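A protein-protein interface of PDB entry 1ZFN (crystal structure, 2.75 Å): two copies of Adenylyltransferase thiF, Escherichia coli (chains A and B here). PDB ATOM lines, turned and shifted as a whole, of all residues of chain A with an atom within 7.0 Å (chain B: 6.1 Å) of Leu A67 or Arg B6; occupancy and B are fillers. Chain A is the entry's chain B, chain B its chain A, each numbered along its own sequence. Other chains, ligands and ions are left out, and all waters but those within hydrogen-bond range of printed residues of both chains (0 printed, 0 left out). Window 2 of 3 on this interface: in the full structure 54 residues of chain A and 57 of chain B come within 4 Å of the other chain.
No position is printed for both chains.
OD1 of Asn B4 sits close to N of Arg B6. OD2 of Asp B99 lies within salt-bridge range of NH1 of Arg B10 (3.4 Å).
Hydrophobic or aromatic side chains of chain B within 4 Å of the printed part of chain A: Pro B98. Among the printed residues, 8 pairs touch across the chains.
Among the printed residues, merely in contact across the chains: Leu A67 with Arg B6 (3.5 Å), Leu A67 with Arg B10 (3.2 Å), Ser A68 with Met B9 (3.5 Å), Ser A68 with Arg B10 (3.8 Å), Leu A70 with Arg B10 (3.3 Å), Gln A71 with Arg B10 (3.6 Å), Thr A78 with Arg B10 (3.2 Å) and Thr A78 with Pro B98 (3.4 Å).
Leu A67 touches two residues of chain B. Printed residues of chain B within 4 Å of Leu A70: Arg B10 (3.3 Å). Asp B5 touches none of the printed residues of chain A. Arg B6 touches just one residue of chain A: Leu A67 (3.5 Å). Of the printed residues of chain A, Met B9 touches Ser A68 (3.5 Å). Of the printed residues of chain A, Arg B10 touches Leu A67 (3.2 Å), Ser A68 (3.8 Å), Leu A70 (3.3 Å), Gln A71 (3.6 Å) and Thr A78 (3.2 Å). Of the printed residues of chain A, Pro B98 touches Thr A78 (3.4 Å). The nearest residue of chain A that does not touch Arg B6 is Ile A81 (5.5 Å).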
ATOM      1  N   VAL A  65     -26.417 -11.612  17.208  1.00  0.00           N
ATOM      2  CA  VAL A  65     -25.442 -10.537  17.289  1.00  0.00           C
ATOM      3  C   VAL A  65     -24.996 -10.153  15.879  1.00  0.00           C
ATOM      4  O   VAL A  65     -25.093 -10.953  14.954  1.00  0.00           O
ATOM      5  CB  VAL A  65     -24.213 -10.973  18.116  1.00  0.00           C
ATOM      6  CG1 VAL A  65     -23.169  -9.877  18.130  1.00  0.00           C
ATOM      7  CG2 VAL A  65     -24.647 -11.296  19.544  1.00  0.00           C
ATOM      8  N   HIS A  66     -24.535  -8.920  15.710  1.00  0.00           N
ATOM      9  CA  HIS A  66     -24.053  -8.451  14.417  1.00  0.00           C
ATOM     10  C   HIS A  66     -22.837  -7.600  14.713  1.00  0.00           C
ATOM     11  O   HIS A  66     -22.747  -7.017  15.789  1.00  0.00           O
ATOM     12  CB  HIS A  66     -25.112  -7.606  13.714  1.00  0.00           C
ATOM     13  CG  HIS A  66     -26.393  -8.332  13.458  1.00  0.00           C
ATOM     14  ND1 HIS A  66     -26.452  -9.517  12.755  1.00  0.00           N
ATOM     15  CD2 HIS A  66     -27.670  -8.034  13.802  1.00  0.00           C
ATOM     16  CE1 HIS A  66     -27.711  -9.916  12.676  1.00  0.00           C
ATOM     17  NE2 HIS A  66     -28.470  -9.034  13.303  1.00  0.00           N
ATOM     18  N   LEU A  67     -21.909  -7.522  13.765  1.00  0.00           N
ATOM     19  CA  LEU A  67     -20.687  -6.747  13.955  1.00  0.00           C
ATOM     20  C   LEU A  67     -20.924  -5.275  14.319  1.00  0.00           C
ATOM     21  O   LEU A  67     -20.185  -4.713  15.133  1.00  0.00           O
ATOM     22  CB  LEU A  67     -19.804  -6.854  12.704  1.00  0.00           C
ATOM     23  CG  LEU A  67     -18.499  -6.034  12.624  1.00  0.00           C
ATOM     24  CD1 LEU A  67     -17.576  -6.284  13.831  1.00  0.00           C
ATOM     25  CD2 LEU A  67     -17.790  -6.386  11.326  1.00  0.00           C
ATOM     26  N   SER A  68     -21.948  -4.658  13.729  1.00  0.00           N
ATOM     27  CA  SER A  68     -22.266  -3.254  13.998  1.00  0.00           C
ATOM     28  C   SER A  68     -22.758  -3.113  15.425  1.00  0.00           C
ATOM     29  O   SER A  68     -22.693  -2.028  16.017  1.00  0.00           O
ATOM     30  CB  SER A  68     -23.368  -2.755  13.063  1.00  0.00           C
ATOM     31  OG  SER A  68     -24.646  -3.220  13.485  1.00  0.00           O
ATOM     32  N   ASN A  69     -23.271  -4.218  15.960  1.00  0.00           N
ATOM     33  CA  ASN A  69     -23.786  -4.240  17.316  1.00  0.00           C
ATOM     34  C   ASN A  69     -22.698  -3.991  18.353  1.00  0.00           C
ATOM     35  O   ASN A  69     -22.920  -3.277  19.331  1.00  0.00           O
ATOM     36  CB  ASN A  69     -24.465  -5.572  17.598  1.00  0.00           C
ATOM     37  CG  ASN A  69     -25.822  -5.675  16.951  1.00  0.00           C
ATOM     38  OD1 ASN A  69     -26.430  -4.661  16.607  1.00  0.00           O
ATOM     39  ND2 ASN A  69     -26.320  -6.899  16.802  1.00  0.00           N
ATOM     40  N   LEU A  70     -21.518  -4.557  18.115  1.00  0.00           N
ATOM     41  CA  LEU A  70     -20.387  -4.432  19.027  1.00  0.00           C
ATOM     42  C   LEU A  70     -19.860  -3.028  19.304  1.00  0.00           C
ATOM     43  O   LEU A  70     -18.809  -2.879  19.929  1.00  0.00           O
ATOM     44  CB  LEU A  70     -19.216  -5.278  18.530  1.00  0.00           C
ATOM     45  CG  LEU A  70     -19.505  -6.723  18.151  1.00  0.00           C
ATOM     46  CD1 LEU A  70     -18.180  -7.415  17.944  1.00  0.00           C
ATOM     47  CD2 LEU A  70     -20.311  -7.413  19.246  1.00  0.00           C
ATOM     48  N   GLN A  71     -20.558  -1.999  18.846  1.00  0.00           N
ATOM     49  CA  GLN A  71     -20.086  -0.646  19.098  1.00  0.00           C
ATOM     50  C   GLN A  71     -20.758  -0.048  20.333  1.00  0.00           C
ATOM     51  O   GLN A  71     -20.271   0.935  20.898  1.00  0.00           O
ATOM     52  CB  GLN A  71     -20.338   0.231  17.869  1.00  0.00           C
ATOM     53  CG  GLN A  71     -20.227   1.711  18.129  1.00  0.00           C
ATOM     54  CD  GLN A  71     -21.581   2.409  18.108  1.00  0.00           C
ATOM     55  OE1 GLN A  71     -22.636   1.768  18.066  1.00  0.00           O
ATOM     56  NE2 GLN A  71     -21.553   3.739  18.137  1.00  0.00           N
ATOM     57  N   THR A  78     -17.060 -10.196  19.609  1.00  0.00           N
ATOM     58  CA  THR A  78     -17.091 -10.509  18.190  1.00  0.00           C
ATOM     59  C   THR A  78     -17.367 -11.991  17.966  1.00  0.00           C
ATOM     60  O   THR A  78     -18.039 -12.371  17.007  1.00  0.00           O
ATOM     61  CB  THR A  78     -15.774 -10.176  17.515  1.00  0.00           C
ATOM     62  OG1 THR A  78     -14.850 -11.230  17.780  1.00  0.00           O
ATOM     63  CG2 THR A  78     -15.210  -8.880  18.052  1.00  0.00           C
ATOM     64  N   ILE A  81     -20.785 -13.045  17.256  1.00  0.00           N
ATOM     65  CA  ILE A  81     -21.299 -12.442  16.026  1.00  0.00           C
ATOM     66  C   ILE A  81     -22.521 -13.070  15.378  1.00  0.00           C
ATOM     67  O   ILE A  81     -23.366 -12.345  14.870  1.00  0.00           O
ATOM     68  CB  ILE A  81     -20.188 -12.308  14.944  1.00  0.00           C
ATOM     69  CG1 ILE A  81     -19.956 -10.830  14.595  1.00  0.00           C
ATOM     70  CG2 ILE A  81     -20.611 -13.015  13.650  1.00  0.00           C
ATOM     71  CD1 ILE A  81     -19.418  -9.983  15.711  1.00  0.00           C
ATOM     72  N   ASN B   4     -10.743   0.860   6.450  1.00  0.00           N
ATOM     73  CA  ASN B   4     -11.252  -0.470   6.048  1.00  0.00           C
ATOM     74  C   ASN B   4     -12.652  -0.546   5.415  1.00  0.00           C
ATOM     75  O   ASN B   4     -13.161   0.431   4.871  1.00  0.00           O
ATOM     76  CB  ASN B   4     -11.198  -1.405   7.272  1.00  0.00           C
ATOM     77  CG  ASN B   4     -11.240  -2.891   6.906  1.00  0.00           C
ATOM     78  OD1 ASN B   4     -11.348  -3.758   7.780  1.00  0.00           O
ATOM     79  ND2 ASN B   4     -11.142  -3.187   5.618  1.00  0.00           N
ATOM     80  N   ASP B   5     -13.237  -1.746   5.477  1.00  0.00           N
ATOM     81  CA  ASP B   5     -14.571  -2.052   4.954  1.00  0.00           C
ATOM     82  C   ASP B   5     -15.270  -2.822   6.090  1.00  0.00           C
ATOM     83  O   ASP B   5     -16.483  -2.709   6.296  1.00  0.00           O
ATOM     84  CB  ASP B   5     -14.472  -2.935   3.692  1.00  0.00           C
ATOM     85  CG  ASP B   5     -15.704  -2.823   2.774  1.00  0.00           C
ATOM     86  OD1 ASP B   5     -15.784  -3.584   1.784  1.00  0.00           O
ATOM     87  OD2 ASP B   5     -16.587  -1.977   3.028  1.00  0.00           O
ATOM     88  N   ARG B   6     -14.485  -3.610   6.822  1.00  0.00           N
ATOM     89  CA  ARG B   6     -14.991  -4.372   7.957  1.00  0.00           C
ATOM     90  C   ARG B   6     -15.207  -3.342   9.053  1.00  0.00           C
ATOM     91  O   ARG B   6     -16.192  -3.389   9.791  1.00  0.00           O
ATOM     92  CB  ARG B   6     -13.956  -5.396   8.412  1.00  0.00           C
ATOM     93  CG  ARG B   6     -14.474  -6.349   9.458  1.00  0.00           C
ATOM     94  CD  ARG B   6     -13.481  -7.456   9.748  1.00  0.00           C
ATOM     95  NE  ARG B   6     -14.164  -8.636  10.271  1.00  0.00           N
ATOM     96  CZ  ARG B   6     -14.733  -8.707  11.469  1.00  0.00           C
ATOM     97  NH1 ARG B   6     -14.698  -7.662  12.288  1.00  0.00           N
ATOM     98  NH2 ARG B   6     -15.358  -9.819  11.839  1.00  0.00           N
ATOM     99  N   ASP B   7     -14.263  -2.409   9.135  1.00  0.00           N
ATOM    100  CA  ASP B   7     -14.305  -1.321  10.098  1.00  0.00           C
ATOM    101  C   ASP B   7     -15.548  -0.478   9.859  1.00  0.00           C
ATOM    102  O   ASP B   7     -16.274  -0.131  10.792  1.00  0.00           O
ATOM    103  CB  ASP B   7     -13.071  -0.438   9.947  1.00  0.00           C
ATOM    104  CG  ASP B   7     -11.823  -1.095  10.475  1.00  0.00           C
ATOM    105  OD1 ASP B   7     -11.814  -2.340  10.583  1.00  0.00           O
ATOM    106  OD2 ASP B   7     -10.850  -0.370  10.773  1.00  0.00           O
ATOM    107  N   PHE B   8     -15.787  -0.142   8.599  1.00  0.00           N
ATOM    108  CA  PHE B   8     -16.945   0.662   8.262  1.00  0.00           C
ATOM    109  C   PHE B   8     -18.218   0.067   8.851  1.00  0.00           C
ATOM    110  O   PHE B   8     -19.087   0.791   9.334  1.00  0.00           O
ATOM    111  CB  PHE B   8     -17.101   0.768   6.746  1.00  0.00           C
ATOM    112  CG  PHE B   8     -18.428   1.320   6.332  1.00  0.00           C
ATOM    113  CD1 PHE B   8     -18.642   2.697   6.297  1.00  0.00           C
ATOM    114  CD2 PHE B   8     -19.493   0.462   6.069  1.00  0.00           C
ATOM    115  CE1 PHE B   8     -19.915   3.219   6.011  1.00  0.00           C
ATOM    116  CE2 PHE B   8     -20.768   0.959   5.782  1.00  0.00           C
ATOM    117  CZ  PHE B   8     -20.984   2.347   5.752  1.00  0.00           C
ATOM    118  N   MET B   9     -18.328  -1.253   8.802  1.00  0.00           N
ATOM    119  CA  MET B   9     -19.508  -1.932   9.305  1.00  0.00           C
ATOM    120  C   MET B   9     -19.582  -1.834  10.820  1.00  0.00           C
ATOM    121  O   MET B   9     -20.600  -1.417  11.379  1.00  0.00           O
ATOM    122  CB  MET B   9     -19.478  -3.392   8.874  1.00  0.00           C
ATOM    123  CG  MET B   9     -20.839  -4.028   8.821  1.00  0.00           C
ATOM    124  SD  MET B   9     -21.971  -3.120   7.750  1.00  0.00           S
ATOM    125  CE  MET B   9     -23.451  -3.161   8.738  1.00  0.00           C
ATOM    126  N   ARG B  10     -18.492  -2.216  11.475  1.00  0.00           N
ATOM    127  CA  ARG B  10     -18.396  -2.173  12.927  1.00  0.00           C
ATOM    128  C   ARG B  10     -18.731  -0.799  13.520  1.00  0.00           C
ATOM    129  O   ARG B  10     -19.492  -0.704  14.486  1.00  0.00           O
ATOM    130  CB  ARG B  10     -16.995  -2.622  13.338  1.00  0.00           C
ATOM    131  CG  ARG B  10     -16.428  -1.974  14.568  1.00  0.00           C
ATOM    132  CD  ARG B  10     -15.258  -2.794  15.053  1.00  0.00           C
ATOM    133  NE  ARG B  10     -15.721  -4.130  15.405  1.00  0.00           N
ATOM    134  CZ  ARG B  10     -14.990  -5.034  16.050  1.00  0.00           C
ATOM    135  NH1 ARG B  10     -13.746  -4.748  16.412  1.00  0.00           N
ATOM    136  NH2 ARG B  10     -15.508  -6.218  16.348  1.00  0.00           N
ATOM    137  N   TYR B  11     -18.183   0.261  12.931  1.00  0.00           N
ATOM    138  CA  TYR B  11     -18.435   1.616  13.413  1.00  0.00           C
ATOM    139  C   TYR B  11     -19.579   2.335  12.676  1.00  0.00           C
ATOM    140  O   TYR B  11     -19.809   3.527  12.881  1.00  0.00           O
ATOM    141  CB  TYR B  11     -17.145   2.435  13.326  1.00  0.00           C
ATOM    142  CG  TYR B  11     -15.958   1.753  13.980  1.00  0.00           C
ATOM    143  CD1 TYR B  11     -14.820   1.440  13.243  1.00  0.00           C
ATOM    144  CD2 TYR B  11     -15.978   1.410  15.332  1.00  0.00           C
ATOM    145  CE1 TYR B  11     -13.728   0.803  13.827  1.00  0.00           C
ATOM    146  CE2 TYR B  11     -14.885   0.766  15.931  1.00  0.00           C
ATOM    147  CZ  TYR B  11     -13.764   0.467  15.171  1.00  0.00           C
ATOM    148  OH  TYR B  11     -12.677  -0.159  15.747  1.00  0.00           O
ATOM    149  N   PRO B  98     -11.088  -6.720  18.491  1.00  0.00           N
ATOM    150  CA  PRO B  98      -9.735  -7.242  18.260  1.00  0.00           C
ATOM    151  C   PRO B  98      -8.858  -6.268  17.484  1.00  0.00           C
ATOM    152  O   PRO B  98      -7.630  -6.285  17.601  1.00  0.00           O
ATOM    153  CB  PRO B  98      -9.984  -8.516  17.455  1.00  0.00           C
ATOM    154  CG  PRO B  98     -11.446  -8.847  17.705  1.00  0.00           C
ATOM    155  CD  PRO B  98     -12.083  -7.495  17.733  1.00  0.00           C
ATOM    156  N   ASP B  99      -9.506  -5.414  16.700  1.00  0.00           N
ATOM    157  CA  ASP B  99      -8.812  -4.444  15.862  1.00  0.00           C
ATOM    158  C   ASP B  99      -8.398  -3.161  16.571  1.00  0.00           C
ATOM    159  O   ASP B  99      -8.260  -2.118  15.928  1.00  0.00           O
ATOM    160  CB  ASP B  99      -9.687  -4.094  14.651  1.00  0.00           C
ATOM    161  CG  ASP B  99     -10.350  -5.320  14.034  1.00  0.00           C
ATOM    162  OD1 ASP B  99      -9.641  -6.318  13.779  1.00  0.00           O
ATOM    163  OD2 ASP B  99     -11.581  -5.282  13.802  1.00  0.00           O
